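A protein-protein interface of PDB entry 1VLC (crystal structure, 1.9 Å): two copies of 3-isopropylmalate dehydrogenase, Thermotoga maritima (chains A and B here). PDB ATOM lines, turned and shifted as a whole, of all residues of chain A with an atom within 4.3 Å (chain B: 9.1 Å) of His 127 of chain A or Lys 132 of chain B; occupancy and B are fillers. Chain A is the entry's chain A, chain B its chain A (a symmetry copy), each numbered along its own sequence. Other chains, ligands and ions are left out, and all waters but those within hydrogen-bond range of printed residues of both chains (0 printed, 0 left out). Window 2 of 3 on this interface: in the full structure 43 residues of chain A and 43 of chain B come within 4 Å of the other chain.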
ATOM      1  N   SER A 124       6.363 -12.723  -8.989  1.00  0.00           N
ATOM      2  CA  SER A 124       7.135 -13.970  -9.031  1.00  0.00           C
ATOM      3  C   SER A 124       8.428 -13.918  -9.825  1.00  0.00           C
ATOM      4  O   SER A 124       9.233 -14.845  -9.736  1.00  0.00           O
ATOM      5  CB  SER A 124       6.262 -15.118  -9.558  1.00  0.00           C
ATOM      6  OG  SER A 124       5.392 -14.650 -10.593  1.00  0.00           O
ATOM      7  N   LEU A 125       8.669 -12.864 -10.599  1.00  0.00           N
ATOM      8  CA  LEU A 125       9.956 -12.738 -11.259  1.00  0.00           C
ATOM      9  C   LEU A 125      10.802 -11.591 -10.724  1.00  0.00           C
ATOM     10  O   LEU A 125      11.674 -11.092 -11.451  1.00  0.00           O
ATOM     11  CB  LEU A 125       9.746 -12.438 -12.742  1.00  0.00           C
ATOM     12  CG  LEU A 125       8.984 -13.461 -13.554  1.00  0.00           C
ATOM     13  CD1 LEU A 125       9.168 -13.091 -15.008  1.00  0.00           C
ATOM     14  CD2 LEU A 125       9.447 -14.885 -13.329  1.00  0.00           C
ATOM     15  N   VAL A 126      10.516 -11.127  -9.509  1.00  0.00           N
ATOM     16  CA  VAL A 126      11.207  -9.957  -8.961  1.00  0.00           C
ATOM     17  C   VAL A 126      12.688 -10.259  -8.888  1.00  0.00           C
ATOM     18  O   VAL A 126      13.520  -9.337  -8.993  1.00  0.00           O
ATOM     19  CB  VAL A 126      10.654  -9.537  -7.553  1.00  0.00           C
ATOM     20  CG1 VAL A 126      11.659  -8.659  -6.781  1.00  0.00           C
ATOM     21  CG2 VAL A 126       9.341  -8.804  -7.657  1.00  0.00           C
ATOM     22  N   HIS A 127      13.027 -11.529  -8.644  1.00  0.00           N
ATOM     23  CA  HIS A 127      14.418 -11.956  -8.545  1.00  0.00           C
ATOM     24  C   HIS A 127      15.171 -11.813  -9.856  1.00  0.00           C
ATOM     25  O   HIS A 127      16.380 -11.828  -9.857  1.00  0.00           O
ATOM     26  CB  HIS A 127      14.484 -13.439  -8.074  1.00  0.00           C
ATOM     27  CG  HIS A 127      13.861 -14.399  -9.038  1.00  0.00           C
ATOM     28  ND1 HIS A 127      12.529 -14.761  -8.977  1.00  0.00           N
ATOM     29  CD2 HIS A 127      14.371 -15.023 -10.128  1.00  0.00           C
ATOM     30  CE1 HIS A 127      12.252 -15.578  -9.979  1.00  0.00           C
ATOM     31  NE2 HIS A 127      13.354 -15.761 -10.686  1.00  0.00           N
ATOM     32  N   VAL A 128      14.453 -11.683 -10.972  1.00  0.00           N
ATOM     33  CA  VAL A 128      15.044 -11.446 -12.306  1.00  0.00           C
ATOM     34  C   VAL A 128      15.297  -9.964 -12.566  1.00  0.00           C
ATOM     35  O   VAL A 128      16.079  -9.622 -13.446  1.00  0.00           O
ATOM     36  CB  VAL A 128      14.079 -11.938 -13.442  1.00  0.00           C
ATOM     37  CG1 VAL A 128      14.671 -11.707 -14.817  1.00  0.00           C
ATOM     38  CG2 VAL A 128      13.741 -13.420 -13.304  1.00  0.00           C
ATOM     39  N   SER A 129      14.608  -9.085 -11.839  1.00  0.00           N
ATOM     40  CA  SER A 129      14.805  -7.654 -11.993  1.00  0.00           C
ATOM     41  C   SER A 129      16.176  -7.247 -11.514  1.00  0.00           C
ATOM     42  O   SER A 129      16.717  -7.848 -10.590  1.00  0.00           O
ATOM     43  CB  SER A 129      13.764  -6.870 -11.199  1.00  0.00           C
ATOM     44  OG  SER A 129      13.979  -5.464 -11.275  1.00  0.00           O
ATOM     45  N   PRO A 130      16.753  -6.225 -12.133  1.00  0.00           N
ATOM     46  CA  PRO A 130      18.012  -5.637 -11.624  1.00  0.00           C
ATOM     47  C   PRO A 130      17.880  -4.827 -10.317  1.00  0.00           C
ATOM     48  O   PRO A 130      18.895  -4.565  -9.637  1.00  0.00           O
ATOM     49  CB  PRO A 130      18.459  -4.721 -12.785  1.00  0.00           C
ATOM     50  CG  PRO A 130      17.295  -4.484 -13.600  1.00  0.00           C
ATOM     51  CD  PRO A 130      16.323  -5.599 -13.382  1.00  0.00           C
ATOM     52  N   LEU A 131      16.652  -4.446  -9.955  1.00  0.00           N
ATOM     53  CA  LEU A 131      16.366  -3.601  -8.790  1.00  0.00           C
ATOM     54  C   LEU A 131      16.135  -4.495  -7.542  1.00  0.00           C
ATOM     55  O   LEU A 131      15.525  -5.558  -7.659  1.00  0.00           O
ATOM     56  CB  LEU A 131      15.096  -2.751  -9.050  1.00  0.00           C
ATOM     57  CG  LEU A 131      15.038  -1.647 -10.122  1.00  0.00           C
ATOM     58  CD1 LEU A 131      13.839  -0.724  -9.863  1.00  0.00           C
ATOM     59  CD2 LEU A 131      16.304  -0.835 -10.090  1.00  0.00           C
ATOM     60  N   LYS A 132      16.578  -4.045  -6.362  1.00  0.00           N
ATOM     61  CA  LYS A 132      16.350  -4.778  -5.102  1.00  0.00           C
ATOM     62  C   LYS A 132      14.840  -4.895  -4.889  1.00  0.00           C
ATOM     63  O   LYS A 132      14.081  -4.027  -5.287  1.00  0.00           O
ATOM     64  CB  LYS A 132      16.951  -4.078  -3.880  1.00  0.00           C
ATOM     65  CG  LYS A 132      18.528  -4.045  -3.752  1.00  0.00           C
ATOM     66  CD  LYS A 132      18.921  -3.767  -2.321  1.00  0.00           C
ATOM     67  CE  LYS A 132      20.378  -3.190  -2.050  1.00  0.00           C
ATOM     68  NZ  LYS A 132      21.521  -3.602  -2.968  1.00  0.00           N
ATOM     69  N   GLU A 133      14.421  -5.959  -4.218  1.00  0.00           N
ATOM     70  CA  GLU A 133      12.997  -6.226  -4.003  1.00  0.00           C
ATOM     71  C   GLU A 133      12.329  -5.066  -3.237  1.00  0.00           C
ATOM     72  O   GLU A 133      11.212  -4.706  -3.542  1.00  0.00           O
ATOM     73  CB  GLU A 133      12.842  -7.542  -3.253  1.00  0.00           C
ATOM     74  N   VAL B 121      30.208   3.085  -6.250  1.00  0.00           N
ATOM     75  CA  VAL B 121      29.432   2.349  -5.263  1.00  0.00           C
ATOM     76  C   VAL B 121      30.494   1.695  -4.346  1.00  0.00           C
ATOM     77  O   VAL B 121      31.312   0.891  -4.779  1.00  0.00           O
ATOM     78  CB  VAL B 121      28.502   1.334  -5.909  1.00  0.00           C
ATOM     79  CG1 VAL B 121      27.741   0.536  -4.822  1.00  0.00           C
ATOM     80  CG2 VAL B 121      27.527   2.021  -6.820  1.00  0.00           C
ATOM     81  N   ARG B 123      31.996  -0.771  -1.722  1.00  0.00           N
ATOM     82  CA  ARG B 123      31.614  -2.145  -1.385  1.00  0.00           C
ATOM     83  C   ARG B 123      30.732  -2.219  -0.117  1.00  0.00           C
ATOM     84  O   ARG B 123      29.745  -2.949  -0.065  1.00  0.00           O
ATOM     85  CB  ARG B 123      32.849  -3.024  -1.209  1.00  0.00           C
ATOM     86  CG  ARG B 123      32.500  -4.511  -0.875  1.00  0.00           C
ATOM     87  CD  ARG B 123      31.513  -5.190  -1.856  1.00  0.00           C
ATOM     88  NE  ARG B 123      32.045  -5.164  -3.221  1.00  0.00           N
ATOM     89  CZ  ARG B 123      31.396  -5.553  -4.323  1.00  0.00           C
ATOM     90  NH1 ARG B 123      30.137  -6.004  -4.271  1.00  0.00           N
ATOM     91  NH2 ARG B 123      32.017  -5.474  -5.498  1.00  0.00           N
ATOM     92  N   VAL B 126      26.825  -1.158  -0.447  1.00  0.00           N
ATOM     93  CA  VAL B 126      26.099  -1.739  -1.580  1.00  0.00           C
ATOM     94  C   VAL B 126      24.646  -1.904  -1.190  1.00  0.00           C
ATOM     95  O   VAL B 126      23.755  -1.844  -2.059  1.00  0.00           O
ATOM     96  CB  VAL B 126      26.709  -3.109  -2.046  1.00  0.00           C
ATOM     97  CG1 VAL B 126      25.701  -3.935  -2.869  1.00  0.00           C
ATOM     98  CG2 VAL B 126      27.967  -2.921  -2.856  1.00  0.00           C
ATOM     99  N   HIS B 127      24.399  -2.176   0.095  1.00  0.00           N
ATOM    100  CA  HIS B 127      23.045  -2.362   0.605  1.00  0.00           C
ATOM    101  C   HIS B 127      22.208  -1.098   0.520  1.00  0.00           C
ATOM    102  O   HIS B 127      21.004  -1.170   0.608  1.00  0.00           O
ATOM    103  CB  HIS B 127      23.098  -2.846   2.084  1.00  0.00           C
ATOM    104  CG  HIS B 127      23.719  -1.851   3.014  1.00  0.00           C
ATOM    105  ND1 HIS B 127      25.072  -1.834   3.295  1.00  0.00           N
ATOM    106  CD2 HIS B 127      23.183  -0.799   3.679  1.00  0.00           C
ATOM    107  CE1 HIS B 127      25.337  -0.823   4.104  1.00  0.00           C
ATOM    108  NE2 HIS B 127      24.208  -0.185   4.360  1.00  0.00           N
ATOM    109  N   VAL B 128      22.849   0.060   0.358  1.00  0.00           N
ATOM    110  CA  VAL B 128      22.165   1.357   0.171  1.00  0.00           C
ATOM    111  C   VAL B 128      21.807   1.611  -1.290  1.00  0.00           C
ATOM    112  O   VAL B 128      20.955   2.444  -1.577  1.00  0.00           O
ATOM    113  CB  VAL B 128      23.088   2.547   0.615  1.00  0.00           C
ATOM    114  CG1 VAL B 128      22.401   3.885   0.433  1.00  0.00           C
ATOM    115  CG2 VAL B 128      23.523   2.420   2.072  1.00  0.00           C
ATOM    116  N   SER B 129      22.485   0.933  -2.217  1.00  0.00           N
ATOM    117  CA  SER B 129      22.192   1.084  -3.631  1.00  0.00           C
ATOM    118  C   SER B 129      20.830   0.524  -3.961  1.00  0.00           C
ATOM    119  O   SER B 129      20.383  -0.433  -3.337  1.00  0.00           O
ATOM    120  CB  SER B 129      23.230   0.359  -4.485  1.00  0.00           C
ATOM    121  OG  SER B 129      22.926   0.430  -5.874  1.00  0.00           O
ATOM    122  N   PRO B 130      20.156   1.114  -4.940  1.00  0.00           N
ATOM    123  CA  PRO B 130      18.897   0.534  -5.456  1.00  0.00           C
ATOM    124  C   PRO B 130      19.058  -0.758  -6.286  1.00  0.00           C
ATOM    125  O   PRO B 130      18.072  -1.496  -6.493  1.00  0.00           O
ATOM    126  CB  PRO B 130      18.327   1.671  -6.332  1.00  0.00           C
ATOM    127  CG  PRO B 130      19.423   2.557  -6.630  1.00  0.00           C
ATOM    128  CD  PRO B 130      20.472   2.391  -5.578  1.00  0.00           C
ATOM    129  N   LEU B 131      20.281  -1.042  -6.744  1.00  0.00           N
ATOM    130  CA  LEU B 131      20.584  -2.182  -7.616  1.00  0.00           C
ATOM    131  C   LEU B 131      20.943  -3.419  -6.750  1.00  0.00           C
ATOM    132  O   LEU B 131      21.608  -3.273  -5.724  1.00  0.00           O
ATOM    133  CB  LEU B 131      21.782  -1.840  -8.537  1.00  0.00           C
ATOM    134  CG  LEU B 131      21.709  -0.760  -9.633  1.00  0.00           C
ATOM    135  CD1 LEU B 131      22.863  -0.940 -10.629  1.00  0.00           C
ATOM    136  CD2 LEU B 131      20.400  -0.864 -10.367  1.00  0.00           C
ATOM    137  N   LYS B 132      20.545  -4.621  -7.184  1.00  0.00           N
ATOM    138  CA  LYS B 132      20.893  -5.870  -6.479  1.00  0.00           C
ATOM    139  C   LYS B 132      22.417  -5.992  -6.455  1.00  0.00           C
ATOM    140  O   LYS B 132      23.097  -5.543  -7.363  1.00  0.00           O
ATOM    141  CB  LYS B 132      20.325  -7.122  -7.154  1.00  0.00           C
ATOM    142  CG  LYS B 132      18.760  -7.345  -7.093  1.00  0.00           C
ATOM    143  CD  LYS B 132      18.437  -8.795  -7.361  1.00  0.00           C
ATOM    144  CE  LYS B 132      16.966  -9.150  -7.852  1.00  0.00           C
ATOM    145  NZ  LYS B 132      15.797  -8.306  -7.364  1.00  0.00           N
ATOM    146  N   GLU B 133      22.939  -6.643  -5.425  1.00  0.00           N
ATOM    147  CA  GLU B 133      24.387  -6.773  -5.246  1.00  0.00           C
ATOM    148  C   GLU B 133      25.029  -7.490  -6.451  1.00  0.00           C
ATOM    149  O   GLU B 133      26.101  -7.115  -6.875  1.00  0.00           O
ATOM    150  CB  GLU B 133      24.667  -7.521  -3.949  1.00  0.00           C
ATOM    151  N   LYS B 134      24.377  -8.507  -7.017  1.00  0.00           N
ATOM    152  CA  LYS B 134      24.963  -9.226  -8.168  1.00  0.00           C
ATOM    153  C   LYS B 134      24.910  -8.375  -9.454  1.00  0.00           C
ATOM    154  O   LYS B 134      25.674  -8.597 -10.399  1.00  0.00           O
ATOM    155  CB  LYS B 134      24.236 -10.537  -8.410  1.00  0.00           C
ATOM    156  N   VAL B 135      23.968  -7.444  -9.516  1.00  0.00           N
ATOM    157  CA  VAL B 135      23.938  -6.519 -10.641  1.00  0.00           C
ATOM    158  C   VAL B 135      25.195  -5.640 -10.552  1.00  0.00           C
ATOM    159  O   VAL B 135      25.917  -5.481 -11.536  1.00  0.00           O
ATOM    160  CB  VAL B 135      22.608  -5.695 -10.708  1.00  0.00           C
ATOM    161  CG2 VAL B 135      22.773  -4.565 -11.708  1.00  0.00           C
ATOM    162  N   ILE B 136      25.486  -5.108  -9.369  1.00  0.00           N
ATOM    163  CA  ILE B 136      26.693  -4.267  -9.181  1.00  0.00           C
ATOM    164  C   ILE B 136      27.974  -5.017  -9.595  1.00  0.00           C
ATOM    165  O   ILE B 136      28.922  -4.440 -10.139  1.00  0.00           O
ATOM    166  CB  ILE B 136      26.757  -3.770  -7.720  1.00  0.00           C
ATOM    167  CG1 ILE B 136      25.627  -2.749  -7.495  1.00  0.00           C
ATOM    168  CG2 ILE B 136      28.118  -3.132  -7.393  1.00  0.00           C
ATOM    169  CD1 ILE B 136      25.284  -2.521  -6.029  1.00  0.00           C
ATOM    170  N   GLY B 137      28.007  -6.325  -9.324  1.00  0.00           N
ATOM    171  CA  GLY B 137      29.054  -7.162  -9.884  1.00  0.00           C
ATOM    172  C   GLY B 137      30.416  -6.849  -9.314  1.00  0.00           C
ATOM    173  O   GLY B 137      30.561  -6.614  -8.110  1.00  0.00           O
ATOM    174  N   SER B 138      31.412  -6.839 -10.202  1.00  0.00           N
ATOM    175  CA  SER B 138      32.779  -6.480  -9.864  1.00  0.00           C
ATOM    176  C   SER B 138      32.942  -5.048  -9.373  1.00  0.00           C
ATOM    177  O   SER B 138      34.020  -4.715  -8.935  1.00  0.00           O
ATOM    178  CB  SER B 138      33.712  -6.697 -11.073  1.00  0.00           C
ATOM    179  OG  SER B 138      33.378  -5.857 -12.172  1.00  0.00           O
ATOM    180  N   VAL B 140      31.125  -0.606  -9.275  1.00  0.00           N
ATOM    181  CA  VAL B 140      30.795   0.552 -10.097  1.00  0.00           C
ATOM    182  C   VAL B 140      31.823   1.648  -9.819  1.00  0.00           C
ATOM    183  O   VAL B 140      32.006   2.043  -8.672  1.00  0.00           O
ATOM    184  CB  VAL B 140      29.381   1.066  -9.819  1.00  0.00           C
ATOM    185  CG1 VAL B 140      29.144   2.436 -10.447  1.00  0.00           C
ATOM    186  CG2 VAL B 140      28.358   0.059 -10.340  1.00  0.00           C
ATOM    187  N   ILE B 238      21.710   0.389 -15.670  1.00  0.00           N
ATOM    188  CA  ILE B 238      20.967  -0.375 -14.709  1.00  0.00           C
ATOM    189  C   ILE B 238      21.373  -1.841 -14.818  1.00  0.00           C
ATOM    190  O   ILE B 238      21.625  -2.474 -13.811  1.00  0.00           O
ATOM    191  CB  ILE B 238      19.455  -0.195 -14.883  1.00  0.00           C
ATOM    192  CG1 ILE B 238      19.081   1.270 -14.630  1.00  0.00           C
ATOM    193  CG2 ILE B 238      18.689  -1.113 -13.935  1.00  0.00           C
ATOM    194  CD1 ILE B 238      17.802   1.681 -15.347  1.00  0.00           C
ATOM    195  N   LEU B 239      21.495  -2.364 -16.034  1.00  0.00           N
ATOM    196  CA  LEU B 239      21.804  -3.789 -16.214  1.00  0.00           C
ATOM    197  C   LEU B 239      23.251  -4.170 -15.996  1.00  0.00           C
ATOM    198  O   LEU B 239      23.509  -5.255 -15.509  1.00  0.00           O
ATOM    199  CB  LEU B 239      21.388  -4.282 -17.590  1.00  0.00           C
ATOM    200  CG  LEU B 239      19.870  -4.296 -17.790  1.00  0.00           C
ATOM    201  CD1 LEU B 239      19.525  -4.538 -19.245  1.00  0.00           C
ATOM    202  CD2 LEU B 239      19.278  -5.391 -16.915  1.00  0.00           C
ATOM    203  N   PRO B 241      26.409  -1.640 -14.983  1.00  0.00           N
ATOM    204  CA  PRO B 241      27.156  -0.405 -14.856  1.00  0.00           C
ATOM    205  C   PRO B 241      28.663  -0.583 -14.724  1.00  0.00           C
ATOM    206  O   PRO B 241      29.407   0.377 -14.968  1.00  0.00           O
ATOM    207  CB  PRO B 241      26.580   0.230 -13.576  1.00  0.00           C
ATOM    208  CG  PRO B 241      25.921  -0.910 -12.839  1.00  0.00           C
ATOM    209  CD  PRO B 241      25.452  -1.823 -13.888  1.00  0.00           C
ATOM    210  N   LEU B 264      22.650   5.406  -8.432  1.00  0.00           N
ATOM    211  CA  LEU B 264      23.297   4.106  -8.155  1.00  0.00           C
ATOM    212  C   LEU B 264      23.895   3.966  -6.759  1.00  0.00           C
ATOM    213  O   LEU B 264      23.753   2.917  -6.162  1.00  0.00           O
ATOM    214  CB  LEU B 264      24.359   3.724  -9.194  1.00  0.00           C
ATOM    215  CG  LEU B 264      23.925   3.728 -10.676  1.00  0.00           C
ATOM    216  CD1 LEU B 264      24.967   3.063 -11.593  1.00  0.00           C
ATOM    217  CD2 LEU B 264      22.545   3.074 -10.852  1.00  0.00           C
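The backbone carbonyl oxygen (O) of Leu 131 of chain B sits at hydrogen-bond distance from the side-chain amino group (NZ) of Lys 132 of chain A, 2.8 Å away. The backbone carbonyl oxygen (O) of Ser 129 of chain A sits close to the side-chain amino group (NZ) of Lys 132 of chain B, at 3.4 Å. N of Lys 132 of chain A lies within hydrogen-bond range of O of Pro 130 of chain B (3.0 Å). The backbone NH (N) of Lys 132 of chain B is in hydrogen-bond range of the backbone carbonyl oxygen (O) of Pro 130 of chain A (3.0 Å). NZ of Lys 132 of chain A lies close to O of Ser 129 of chain B (3.4 Å). O of Val 126 of chain A is in hydrogen-bond range of NZ of Lys 132 of chain B, 3.0 Å away. NZ of Lys 132 of chain A lies within hydrogen-bond range of O of Val 126 of chain B (3.0 Å). The backbone carbonyl oxygen (O) of Leu 131 of chain A is in hydrogen-bond range of the side-chain amino group (NZ) of Lys 132 of chain B.
The backbone carbonyl oxygen of Leu 264 of chain B lies within hydrogen-bond range of the side-chain hydroxyl of Ser 129 of chain B (2.6 Å). The side-chain hydroxyl (OG) of Ser 129 of chain A lies within hydrogen-bond range of the backbone NH (N) of Leu 131 of chain A (3.2 Å). ND1 of His 127 of chain A sits close to O of Ser 124 of chain A, at 3.4 Å. The side-chain hydroxyl (OG) of Ser 129 of chain B sits at hydrogen-bond distance from the backbone NH (N) of Leu 131 of chain B (3.1 Å).
Among the printed residues, pairs that only touch across the chains: His 127 of chain A with Lys 132 of chain B (3.4 Å), Pro 130 of chain A with Leu 131 of chain B (3.6 Å), Pro 130 of chain A with Ile 238 of chain B (3.7 Å), Pro 130 of chain A with Leu 239 of chain B (3.97 Å), Leu 131 of chain A with Pro 130 of chain B (3.6 Å) and Lys 132 of chain A with His 127 of chain B (3.4 Å).
Printed residues of chain B within 4 Å of His 127 of chain A: Lys 132 (3.4 Å). Lys 132 of chain B touches five residues of chain A. Val 126 of chain A touches one residue of chain B. No residue of chain B comes within 4 Å of Val 128 of chain A. Of the printed residues of chain A, Ser 129 of chain B touches Lys 132 (3.0 Å). Of the printed residues of chain A, Leu 131 of chain B touches Pro 130 (3.6 Å) and Lys 132 (2.8 Å). Of the printed residues of chain A, Leu 239 of chain B touches Pro 130. Leu 264 of chain B touches none of the printed residues of chain A. Ser 138 of chain B touches none of the printed residues of chain A. The nearest residue of chain A that does not touch Lys 132 of chain B is Lys 132 of chain A (4.02 Å).
Of the 20 printed residues of chain B, 8 touch a printed residue of chain A. Of the 10 printed residues of chain A, 6 touch a printed residue of chain B. Printed residues of chain A that touch a printed residue of chain B: Val 126, His 127, Ser 129, Pro 130, Leu 131 and Lys 132. Hydrophobic or aromatic side chains of chain A within 4 Å of the printed part of chain B: Pro 130. Among the printed residues, 14 pairs touch across the chains.
His 127 of chain A touches Lys 132 of chain B, and with the chains exchanged Lys 132 of chain A touches His 127 of chain B. Ser 129 of chain A touches Lys 132 of chain B, and with the chains exchanged Lys 132 of chain A touches Ser 129 of chain B. Pro 130 of chain A touches Leu 131 of chain B, and with the chains exchanged Leu 131 of chain A touches Pro 130 of chain B. Leu 131 of chain A touches Lys 132 of chain B, and with the chains exchanged Lys 132 of chain A touches Leu 131 of chain B. 8 positions are printed for both chains.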
